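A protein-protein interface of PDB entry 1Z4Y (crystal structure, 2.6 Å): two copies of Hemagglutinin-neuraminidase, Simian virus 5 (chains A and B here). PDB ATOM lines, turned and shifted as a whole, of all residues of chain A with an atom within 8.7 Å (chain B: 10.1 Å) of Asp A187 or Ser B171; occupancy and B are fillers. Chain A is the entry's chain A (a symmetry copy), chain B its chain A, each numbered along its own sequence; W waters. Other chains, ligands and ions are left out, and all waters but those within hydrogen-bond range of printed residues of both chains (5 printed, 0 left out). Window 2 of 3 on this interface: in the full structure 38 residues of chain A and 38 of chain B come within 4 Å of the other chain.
OG of Ser B171 sits at hydrogen-bond distance from OG of Ser A186 (2.8 Å).
O of Glu B168 is in hydrogen-bond range of N of Phe B176.
The backbone NH (N) of Val A189 is in hydrogen-bond range of the side-chain carboxylate (OD1) of Asp A187.
The side-chain hydroxyl (OG) of Ser A186 sits at hydrogen-bond distance from the side-chain amide oxygen (OD1) of Asn A159 (3.1 Å).
ND2 of Asn A159 is in hydrogen-bond range of OH of Tyr A184 (3.0 Å).
The side-chain hydroxyl (OG1) of Thr B170 sits close to the backbone NH (N) of Ala B172.
O of Phe B174 is in hydrogen-bond range of OG1 of Thr B170.
Among the printed residues, merely in contact across the chains: Tyr A184 with Phe B176 (3.2 Å), Leu A149 with Asn B114 (3.3 Å), Ser A186 with Thr B170 (3.6 Å), Tyr A184 with Pro B116 (3.6 Å), Leu A149 with Phe B174 (3.8 Å), Asp A187 with Ser B171 (3.9 Å) and Tyr A184 with Thr B170 (3.9 Å).
Of the printed residues of chain B, Tyr A184 touches Pro B116, Thr B170 and Phe B176.
Of chain B, only Thr B170 (3.6 Å) and Ser B171 (2.8 Å) come within 4 Å of Ser A186.
Of chain B, only Ser B171 (3.9 Å) comes within 4 Å of Asp A187.
No residue of chain B comes within 4 Å of Val A189.
Arg A227 touches none of the printed residues of chain B.
Of the printed residues of chain A, Asn B114 touches Leu A149 (3.3 Å).
Of the printed residues of chain A, Pro B116 touches Tyr A184.
Of the printed residues of chain A, Ser B171 touches Ser A186 (2.8 Å) and Asp A187 (3.9 Å).
Of the printed residues of chain A, Phe B174 touches Leu A149.
Printed residues of chain A that touch a printed residue of chain B: Leu A149, Tyr A184, Ser A186 and Asp A187.
Hydrophobic or aromatic side chains of chain B within 4 Å of the printed part of chain A: Pro B116, Phe B174 and Phe B176.
Among the printed residues, 8 pairs touch across the chains.
Among the printed residues, no Asp or Glu carboxylate lies within 4 Å of a Lys or Arg side-chain nitrogen of the other chain.
No position is printed for both chains.
Water W4 lies within hydrogen-bond range of OH of Tyr A184 (2.7 Å) and O of Asn B114 (2.8 Å).
Water W2 lies within hydrogen-bond range of OG of Ser B171 (2.8 Å), OD1 of Asn A159 (2.8 Å) and N of Gly A188 (3.2 Å).
Water W1 lies within hydrogen-bond range of the side-chain carboxylate of Glu B168 (2.9 Å) and the backbone carbonyl oxygen of Tyr A184 (3.1 Å).
Water W3 bridges the side-chain carboxylate (OE2) of Glu B168 (3.0 Å) and the backbone NH (N) of Tyr A184 (3.1 Å).
Water W5 lies within hydrogen-bond range of OG of Ser B171 and ND2 of Asn A159.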
ATOM      1  N   LEU A 149      13.546 -23.025  -5.123  1.00  0.00           N
ATOM      2  CA  LEU A 149      13.181 -21.636  -4.848  1.00  0.00           C
ATOM      3  C   LEU A 149      14.225 -20.705  -4.211  1.00  0.00           C
ATOM      4  O   LEU A 149      14.332 -19.540  -4.600  1.00  0.00           O
ATOM      5  CB  LEU A 149      11.875 -21.603  -4.039  1.00  0.00           C
ATOM      6  CG  LEU A 149      10.665 -22.286  -4.707  1.00  0.00           C
ATOM      7  CD1 LEU A 149       9.385 -21.964  -3.919  1.00  0.00           C
ATOM      8  CD2 LEU A 149      10.523 -21.810  -6.163  1.00  0.00           C
ATOM      9  N   SER A 158      12.127 -29.124  -3.922  1.00  0.00           N
ATOM     10  CA  SER A 158      12.349 -28.720  -5.310  1.00  0.00           C
ATOM     11  C   SER A 158      11.234 -29.141  -6.258  1.00  0.00           C
ATOM     12  O   SER A 158      10.410 -29.987  -5.931  1.00  0.00           O
ATOM     13  CB  SER A 158      13.657 -29.308  -5.841  1.00  0.00           C
ATOM     14  OG  SER A 158      13.509 -30.687  -6.126  1.00  0.00           O
ATOM     15  N   ASN A 159      11.235 -28.541  -7.444  1.00  0.00           N
ATOM     16  CA  ASN A 159      10.260 -28.859  -8.473  1.00  0.00           C
ATOM     17  C   ASN A 159      11.020 -29.216  -9.736  1.00  0.00           C
ATOM     18  O   ASN A 159      12.197 -28.888  -9.859  1.00  0.00           O
ATOM     19  CB  ASN A 159       9.339 -27.671  -8.728  1.00  0.00           C
ATOM     20  CG  ASN A 159       8.516 -27.320  -7.518  1.00  0.00           C
ATOM     21  OD1 ASN A 159       8.114 -28.213  -6.764  1.00  0.00           O
ATOM     22  ND2 ASN A 159       8.248 -26.039  -7.320  1.00  0.00           N
ATOM     23  N   GLN A 160      10.348 -29.886 -10.666  1.00  0.00           N
ATOM     24  CA  GLN A 160      10.989 -30.315 -11.896  1.00  0.00           C
ATOM     25  C   GLN A 160      10.229 -29.803 -13.110  1.00  0.00           C
ATOM     26  O   GLN A 160       9.083 -30.184 -13.329  1.00  0.00           O
ATOM     27  CB  GLN A 160      11.039 -31.839 -11.921  1.00  0.00           C
ATOM     28  CG  GLN A 160      11.900 -32.453 -13.004  1.00  0.00           C
ATOM     29  CD  GLN A 160      13.371 -32.240 -12.750  1.00  0.00           C
ATOM     30  OE1 GLN A 160      13.818 -32.240 -11.608  1.00  0.00           O
ATOM     31  NE2 GLN A 160      14.138 -32.078 -13.816  1.00  0.00           N
ATOM     32  N   TYR A 184       5.128 -28.690 -15.027  1.00  0.00           N
ATOM     33  CA  TYR A 184       5.901 -28.317 -13.853  1.00  0.00           C
ATOM     34  C   TYR A 184       5.491 -29.252 -12.728  1.00  0.00           C
ATOM     35  O   TYR A 184       4.419 -29.100 -12.153  1.00  0.00           O
ATOM     36  CB  TYR A 184       5.620 -26.854 -13.485  1.00  0.00           C
ATOM     37  CG  TYR A 184       6.563 -26.247 -12.468  1.00  0.00           C
ATOM     38  CD1 TYR A 184       7.946 -26.468 -12.539  1.00  0.00           C
ATOM     39  CD2 TYR A 184       6.078 -25.410 -11.459  1.00  0.00           C
ATOM     40  CE1 TYR A 184       8.816 -25.868 -11.633  1.00  0.00           C
ATOM     41  CE2 TYR A 184       6.938 -24.804 -10.548  1.00  0.00           C
ATOM     42  CZ  TYR A 184       8.305 -25.035 -10.639  1.00  0.00           C
ATOM     43  OH  TYR A 184       9.152 -24.425  -9.738  1.00  0.00           O
ATOM     44  N   LEU A 185       6.330 -30.243 -12.444  1.00  0.00           N
ATOM     45  CA  LEU A 185       6.042 -31.194 -11.388  1.00  0.00           C
ATOM     46  C   LEU A 185       6.380 -30.533 -10.066  1.00  0.00           C
ATOM     47  O   LEU A 185       7.541 -30.462  -9.653  1.00  0.00           O
ATOM     48  CB  LEU A 185       6.866 -32.462 -11.571  1.00  0.00           C
ATOM     49  CG  LEU A 185       6.783 -33.058 -12.976  1.00  0.00           C
ATOM     50  CD1 LEU A 185       7.588 -34.352 -13.047  1.00  0.00           C
ATOM     51  CD2 LEU A 185       5.330 -33.304 -13.326  1.00  0.00           C
ATOM     52  N   SER A 186       5.344 -30.028  -9.417  1.00  0.00           N
ATOM     53  CA  SER A 186       5.482 -29.346  -8.144  1.00  0.00           C
ATOM     54  C   SER A 186       4.431 -29.935  -7.221  1.00  0.00           C
ATOM     55  O   SER A 186       3.266 -29.551  -7.283  1.00  0.00           O
ATOM     56  CB  SER A 186       5.238 -27.853  -8.349  1.00  0.00           C
ATOM     57  OG  SER A 186       5.232 -27.166  -7.118  1.00  0.00           O
ATOM     58  N   ASP A 187       4.833 -30.870  -6.368  1.00  0.00           N
ATOM     59  CA  ASP A 187       3.874 -31.507  -5.483  1.00  0.00           C
ATOM     60  C   ASP A 187       4.451 -32.043  -4.179  1.00  0.00           C
ATOM     61  O   ASP A 187       3.836 -32.889  -3.537  1.00  0.00           O
ATOM     62  CB  ASP A 187       3.181 -32.653  -6.224  1.00  0.00           C
ATOM     63  CG  ASP A 187       4.128 -33.792  -6.557  1.00  0.00           C
ATOM     64  OD1 ASP A 187       5.323 -33.701  -6.203  1.00  0.00           O
ATOM     65  OD2 ASP A 187       3.679 -34.783  -7.168  1.00  0.00           O
ATOM     66  N   GLY A 188       5.626 -31.571  -3.781  1.00  0.00           N
ATOM     67  CA  GLY A 188       6.198 -32.061  -2.541  1.00  0.00           C
ATOM     68  C   GLY A 188       7.154 -33.243  -2.661  1.00  0.00           C
ATOM     69  O   GLY A 188       7.880 -33.538  -1.711  1.00  0.00           O
ATOM     70  N   VAL A 189       7.152 -33.939  -3.797  1.00  0.00           N
ATOM     71  CA  VAL A 189       8.077 -35.054  -3.983  1.00  0.00           C
ATOM     72  C   VAL A 189       9.383 -34.499  -4.542  1.00  0.00           C
ATOM     73  O   VAL A 189       9.406 -33.932  -5.629  1.00  0.00           O
ATOM     74  CB  VAL A 189       7.524 -36.100  -4.958  1.00  0.00           C
ATOM     75  CG1 VAL A 189       8.590 -37.145  -5.252  1.00  0.00           C
ATOM     76  CG2 VAL A 189       6.305 -36.767  -4.347  1.00  0.00           C
ATOM     77  N   ASN A 190      10.465 -34.671  -3.796  1.00  0.00           N
ATOM     78  CA  ASN A 190      11.771 -34.153  -4.191  1.00  0.00           C
ATOM     79  C   ASN A 190      12.486 -35.023  -5.236  1.00  0.00           C
ATOM     80  O   ASN A 190      13.383 -35.807  -4.910  1.00  0.00           O
ATOM     81  CB  ASN A 190      12.633 -33.992  -2.935  1.00  0.00           C
ATOM     82  CG  ASN A 190      13.708 -32.938  -3.089  1.00  0.00           C
ATOM     83  OD1 ASN A 190      13.555 -31.975  -3.837  1.00  0.00           O
ATOM     84  ND2 ASN A 190      14.801 -33.101  -2.353  1.00  0.00           N
ATOM     85  N   ARG A 191      12.067 -34.872  -6.490  1.00  0.00           N
ATOM     86  CA  ARG A 191      12.643 -35.604  -7.612  1.00  0.00           C
ATOM     87  C   ARG A 191      13.957 -34.943  -8.018  1.00  0.00           C
ATOM     88  O   ARG A 191      13.979 -33.760  -8.362  1.00  0.00           O
ATOM     89  CB  ARG A 191      11.653 -35.612  -8.784  1.00  0.00           C
ATOM     90  CG  ARG A 191      10.617 -36.734  -8.694  1.00  0.00           C
ATOM     91  CD  ARG A 191       9.464 -36.554  -9.659  1.00  0.00           C
ATOM     92  NE  ARG A 191       8.599 -35.490  -9.190  1.00  0.00           N
ATOM     93  CZ  ARG A 191       7.334 -35.647  -8.812  1.00  0.00           C
ATOM     94  NH1 ARG A 191       6.748 -36.832  -8.848  1.00  0.00           N
ATOM     95  NH2 ARG A 191       6.658 -34.601  -8.372  1.00  0.00           N
ATOM     96  N   VAL A 209      13.975 -40.042  -5.449  1.00  0.00           N
ATOM     97  CA  VAL A 209      13.464 -39.099  -4.460  1.00  0.00           C
ATOM     98  C   VAL A 209      14.463 -38.881  -3.332  1.00  0.00           C
ATOM     99  O   VAL A 209      14.714 -39.774  -2.513  1.00  0.00           O
ATOM    100  CB  VAL A 209      12.128 -39.587  -3.875  1.00  0.00           C
ATOM    101  CG1 VAL A 209      11.494 -38.497  -3.036  1.00  0.00           C
ATOM    102  CG2 VAL A 209      11.202 -40.002  -5.002  1.00  0.00           C
ATOM    103  N   ARG A 227      11.693 -43.436  -9.323  1.00  0.00           N
ATOM    104  CA  ARG A 227      10.462 -43.188 -10.070  1.00  0.00           C
ATOM    105  C   ARG A 227      10.685 -42.934 -11.550  1.00  0.00           C
ATOM    106  O   ARG A 227      11.677 -42.321 -11.939  1.00  0.00           O
ATOM    107  CB  ARG A 227       9.727 -41.982  -9.501  1.00  0.00           C
ATOM    108  CG  ARG A 227       9.339 -42.097  -8.048  1.00  0.00           C
ATOM    109  CD  ARG A 227       8.628 -40.839  -7.579  1.00  0.00           C
ATOM    110  NE  ARG A 227       8.035 -41.034  -6.261  1.00  0.00           N
ATOM    111  CZ  ARG A 227       6.775 -40.748  -5.959  1.00  0.00           C
ATOM    112  NH1 ARG A 227       5.974 -40.248  -6.887  1.00  0.00           N
ATOM    113  NH2 ARG A 227       6.312 -40.970  -4.734  1.00  0.00           N
ATOM    114  N   ILE A 229       8.499 -41.369 -14.730  1.00  0.00           N
ATOM    115  CA  ILE A 229       7.285 -40.664 -15.121  1.00  0.00           C
ATOM    116  C   ILE A 229       7.173 -40.630 -16.648  1.00  0.00           C
ATOM    117  O   ILE A 229       8.120 -40.252 -17.339  1.00  0.00           O
ATOM    118  CB  ILE A 229       7.294 -39.177 -14.609  1.00  0.00           C
ATOM    119  CG1 ILE A 229       7.696 -39.107 -13.134  1.00  0.00           C
ATOM    120  CG2 ILE A 229       5.918 -38.560 -14.749  1.00  0.00           C
ATOM    121  CD1 ILE A 229       9.199 -38.929 -12.890  1.00  0.00           C
ATOM    122  N   GLU A 239       3.044 -41.804 -13.481  1.00  0.00           N
ATOM    123  CA  GLU A 239       4.250 -41.908 -12.685  1.00  0.00           C
ATOM    124  C   GLU A 239       4.215 -43.215 -11.900  1.00  0.00           C
ATOM    125  O   GLU A 239       3.180 -43.581 -11.350  1.00  0.00           O
ATOM    126  CB  GLU A 239       4.371 -40.718 -11.728  1.00  0.00           C
ATOM    127  CG  GLU A 239       5.554 -40.846 -10.773  1.00  0.00           C
ATOM    128  CD  GLU A 239       5.919 -39.542 -10.090  1.00  0.00           C
ATOM    129  OE1 GLU A 239       5.011 -38.864  -9.565  1.00  0.00           O
ATOM    130  OE2 GLU A 239       7.124 -39.202 -10.074  1.00  0.00           O
ATOM    131  N   ARG B  89      -8.769 -22.036  -9.556  1.00  0.00           N
ATOM    132  CA  ARG B  89      -8.333 -21.048  -8.590  1.00  0.00           C
ATOM    133  C   ARG B  89      -8.178 -19.648  -9.170  1.00  0.00           C
ATOM    134  O   ARG B  89      -8.016 -18.682  -8.429  1.00  0.00           O
ATOM    135  CB  ARG B  89      -7.019 -21.492  -7.959  1.00  0.00           C
ATOM    136  CG  ARG B  89      -7.196 -22.632  -6.982  1.00  0.00           C
ATOM    137  CD  ARG B  89      -6.474 -22.305  -5.701  1.00  0.00           C
ATOM    138  NE  ARG B  89      -5.403 -23.251  -5.429  1.00  0.00           N
ATOM    139  CZ  ARG B  89      -4.248 -22.929  -4.869  1.00  0.00           C
ATOM    140  NH1 ARG B  89      -3.997 -21.674  -4.518  1.00  0.00           N
ATOM    141  NH2 ARG B  89      -3.341 -23.873  -4.658  1.00  0.00           N
ATOM    142  N   TYR B  90      -8.254 -19.537 -10.490  1.00  0.00           N
ATOM    143  CA  TYR B  90      -8.086 -18.245 -11.132  1.00  0.00           C
ATOM    144  C   TYR B  90      -9.226 -17.827 -12.058  1.00  0.00           C
ATOM    145  O   TYR B  90      -9.424 -16.630 -12.280  1.00  0.00           O
ATOM    146  CB  TYR B  90      -6.775 -18.230 -11.929  1.00  0.00           C
ATOM    147  CG  TYR B  90      -5.591 -18.752 -11.156  1.00  0.00           C
ATOM    148  CD1 TYR B  90      -5.105 -18.067 -10.049  1.00  0.00           C
ATOM    149  CD2 TYR B  90      -4.966 -19.946 -11.521  1.00  0.00           C
ATOM    150  CE1 TYR B  90      -4.026 -18.552  -9.321  1.00  0.00           C
ATOM    151  CE2 TYR B  90      -3.883 -20.440 -10.799  1.00  0.00           C
ATOM    152  CZ  TYR B  90      -3.420 -19.739  -9.702  1.00  0.00           C
ATOM    153  OH  TYR B  90      -2.353 -20.216  -8.977  1.00  0.00           O
ATOM    154  N   ASN B 114       9.697 -16.882  -7.016  1.00  0.00           N
ATOM    155  CA  ASN B 114      10.382 -17.514  -8.138  1.00  0.00           C
ATOM    156  C   ASN B 114       9.601 -18.586  -8.880  1.00  0.00           C
ATOM    157  O   ASN B 114       9.362 -19.665  -8.349  1.00  0.00           O
ATOM    158  CB  ASN B 114      11.700 -18.129  -7.678  1.00  0.00           C
ATOM    159  CG  ASN B 114      12.507 -18.677  -8.830  1.00  0.00           C
ATOM    160  OD1 ASN B 114      13.094 -17.923  -9.606  1.00  0.00           O
ATOM    161  ND2 ASN B 114      12.519 -19.991  -8.970  1.00  0.00           N
ATOM    162  N   PRO B 116       9.004 -20.467 -13.032  1.00  0.00           N
ATOM    163  CA  PRO B 116       9.719 -20.617 -14.303  1.00  0.00           C
ATOM    164  C   PRO B 116       9.190 -19.539 -15.249  1.00  0.00           C
ATOM    165  O   PRO B 116       7.980 -19.391 -15.403  1.00  0.00           O
ATOM    166  CB  PRO B 116       9.322 -22.018 -14.765  1.00  0.00           C
ATOM    167  CG  PRO B 116       9.067 -22.739 -13.478  1.00  0.00           C
ATOM    168  CD  PRO B 116       8.301 -21.714 -12.678  1.00  0.00           C
ATOM    169  N   GLU B 168      -1.801 -22.070 -13.322  1.00  0.00           N
ATOM    170  CA  GLU B 168      -2.111 -23.153 -12.402  1.00  0.00           C
ATOM    171  C   GLU B 168      -1.237 -23.020 -11.170  1.00  0.00           C
ATOM    172  O   GLU B 168      -0.094 -22.590 -11.253  1.00  0.00           O
ATOM    173  CB  GLU B 168      -1.879 -24.514 -13.048  1.00  0.00           C
ATOM    174  CG  GLU B 168      -0.455 -24.773 -13.440  1.00  0.00           C
ATOM    175  CD  GLU B 168      -0.243 -26.203 -13.883  1.00  0.00           C
ATOM    176  OE1 GLU B 168      -1.076 -26.713 -14.671  1.00  0.00           O
ATOM    177  OE2 GLU B 168       0.761 -26.815 -13.452  1.00  0.00           O
ATOM    178  N   PRO B 169      -1.770 -23.399 -10.006  1.00  0.00           N
ATOM    179  CA  PRO B 169      -1.037 -23.311  -8.742  1.00  0.00           C
ATOM    180  C   PRO B 169       0.065 -24.337  -8.554  1.00  0.00           C
ATOM    181  O   PRO B 169      -0.044 -25.475  -9.006  1.00  0.00           O
ATOM    182  CB  PRO B 169      -2.139 -23.461  -7.706  1.00  0.00           C
ATOM    183  CG  PRO B 169      -3.075 -24.430  -8.383  1.00  0.00           C
ATOM    184  CD  PRO B 169      -3.134 -23.917  -9.798  1.00  0.00           C
ATOM    185  N   THR B 170       1.130 -23.914  -7.881  1.00  0.00           N
ATOM    186  CA  THR B 170       2.265 -24.778  -7.585  1.00  0.00           C
ATOM    187  C   THR B 170       2.104 -25.185  -6.131  1.00  0.00           C
ATOM    188  O   THR B 170       1.264 -24.641  -5.429  1.00  0.00           O
ATOM    189  CB  THR B 170       3.602 -24.034  -7.740  1.00  0.00           C
ATOM    190  OG1 THR B 170       3.734 -23.056  -6.702  1.00  0.00           O
ATOM    191  CG2 THR B 170       3.662 -23.334  -9.077  1.00  0.00           C
ATOM    192  N   SER B 171       2.913 -26.128  -5.667  1.00  0.00           N
ATOM    193  CA  SER B 171       2.788 -26.572  -4.288  1.00  0.00           C
ATOM    194  C   SER B 171       3.140 -25.500  -3.255  1.00  0.00           C
ATOM    195  O   SER B 171       2.890 -25.687  -2.066  1.00  0.00           O
ATOM    196  CB  SER B 171       3.635 -27.828  -4.063  1.00  0.00           C
ATOM    197  OG  SER B 171       5.000 -27.582  -4.324  1.00  0.00           O
ATOM    198  N   ALA B 172       3.713 -24.383  -3.703  1.00  0.00           N
ATOM    199  CA  ALA B 172       4.081 -23.288  -2.799  1.00  0.00           C
ATOM    200  C   ALA B 172       2.891 -22.357  -2.655  1.00  0.00           C
ATOM    201  O   ALA B 172       2.876 -21.461  -1.809  1.00  0.00           O
ATOM    202  CB  ALA B 172       5.271 -22.520  -3.343  1.00  0.00           C
ATOM    203  N   GLY B 173       1.891 -22.580  -3.496  1.00  0.00           N
ATOM    204  CA  GLY B 173       0.699 -21.768  -3.456  1.00  0.00           C
ATOM    205  C   GLY B 173       0.647 -20.749  -4.572  1.00  0.00           C
ATOM    206  O   GLY B 173      -0.430 -20.427  -5.058  1.00  0.00           O
ATOM    207  N   PHE B 174       1.795 -20.229  -4.992  1.00  0.00           N
ATOM    208  CA  PHE B 174       1.756 -19.237  -6.049  1.00  0.00           C
ATOM    209  C   PHE B 174       1.684 -19.828  -7.452  1.00  0.00           C
ATOM    210  O   PHE B 174       1.961 -21.004  -7.660  1.00  0.00           O
ATOM    211  CB  PHE B 174       2.891 -18.208  -5.889  1.00  0.00           C
ATOM    212  CG  PHE B 174       4.264 -18.787  -5.790  1.00  0.00           C
ATOM    213  CD1 PHE B 174       4.961 -19.166  -6.937  1.00  0.00           C
ATOM    214  CD2 PHE B 174       4.903 -18.861  -4.555  1.00  0.00           C
ATOM    215  CE1 PHE B 174       6.283 -19.602  -6.855  1.00  0.00           C
ATOM    216  CE2 PHE B 174       6.216 -19.293  -4.461  1.00  0.00           C
ATOM    217  CZ  PHE B 174       6.911 -19.664  -5.613  1.00  0.00           C
ATOM    218  N   PRO B 175       1.273 -19.006  -8.432  1.00  0.00           N
ATOM    219  CA  PRO B 175       1.107 -19.346  -9.849  1.00  0.00           C
ATOM    220  C   PRO B 175       2.290 -19.875 -10.635  1.00  0.00           C
ATOM    221  O   PRO B 175       3.449 -19.752 -10.247  1.00  0.00           O
ATOM    222  CB  PRO B 175       0.598 -18.042 -10.468  1.00  0.00           C
ATOM    223  CG  PRO B 175       0.020 -17.297  -9.326  1.00  0.00           C
ATOM    224  CD  PRO B 175       1.001 -17.575  -8.230  1.00  0.00           C
ATOM    225  N   PHE B 176       1.945 -20.464 -11.771  1.00  0.00           N
ATOM    226  CA  PHE B 176       2.896 -20.994 -12.719  1.00  0.00           C
ATOM    227  C   PHE B 176       2.225 -20.822 -14.064  1.00  0.00           C
ATOM    228  O   PHE B 176       1.223 -21.466 -14.342  1.00  0.00           O
ATOM    229  CB  PHE B 176       3.180 -22.475 -12.479  1.00  0.00           C
ATOM    230  CG  PHE B 176       3.749 -23.180 -13.685  1.00  0.00           C
ATOM    231  CD1 PHE B 176       4.811 -22.628 -14.395  1.00  0.00           C
ATOM    232  CD2 PHE B 176       3.204 -24.378 -14.130  1.00  0.00           C
ATOM    233  CE1 PHE B 176       5.331 -23.262 -15.529  1.00  0.00           C
ATOM    234  CE2 PHE B 176       3.719 -25.022 -15.263  1.00  0.00           C
ATOM    235  CZ  PHE B 176       4.780 -24.459 -15.962  1.00  0.00           C
ATOM    236  N   ASP B 498      -6.207 -15.352  -6.585  1.00  0.00           N
ATOM    237  CA  ASP B 498      -6.332 -16.774  -6.310  1.00  0.00           C
ATOM    238  C   ASP B 498      -7.571 -16.829  -5.423  1.00  0.00           C
ATOM    239  O   ASP B 498      -7.517 -16.492  -4.246  1.00  0.00           O
ATOM    240  CB  ASP B 498      -5.116 -17.285  -5.534  1.00  0.00           C
ATOM    241  CG  ASP B 498      -4.992 -18.788  -5.576  1.00  0.00           C
ATOM    242  OD1 ASP B 498      -5.939 -19.487  -5.151  1.00  0.00           O
ATOM    243  OD2 ASP B 498      -3.934 -19.267  -6.041  1.00  0.00           O
ATOM    244  N   TYR B 505      -2.020 -11.606  -6.986  1.00  0.00           N
ATOM    245  CA  TYR B 505      -0.672 -11.693  -7.501  1.00  0.00           C
ATOM    246  C   TYR B 505      -0.647 -10.770  -8.684  1.00  0.00           C
ATOM    247  O   TYR B 505      -1.610 -10.695  -9.450  1.00  0.00           O
ATOM    248  CB  TYR B 505      -0.331 -13.104  -7.973  1.00  0.00           C
ATOM    249  CG  TYR B 505      -0.237 -14.112  -6.866  1.00  0.00           C
ATOM    250  CD1 TYR B 505      -1.376 -14.757  -6.396  1.00  0.00           C
ATOM    251  CD2 TYR B 505       0.985 -14.405  -6.269  1.00  0.00           C
ATOM    252  CE1 TYR B 505      -1.301 -15.672  -5.358  1.00  0.00           C
ATOM    253  CE2 TYR B 505       1.074 -15.319  -5.227  1.00  0.00           C
ATOM    254  CZ  TYR B 505      -0.079 -15.950  -4.776  1.00  0.00           C
ATOM    255  OH  TYR B 505      -0.025 -16.858  -3.746  1.00  0.00           O
HETATM  256  O   HOH W   1       2.261 -27.224 -11.041  1.00  0.00           O
HETATM  257  O   HOH W   2       7.435 -28.901  -4.097  1.00  0.00           O
HETATM  258  O   HOH W   3       2.032 -29.079 -15.025  1.00  0.00           O
HETATM  259  O   HOH W   4       8.043 -21.993  -9.180  1.00  0.00           O
HETATM  260  O   HOH W   5       7.042 -25.236  -4.462  1.00  0.00           O
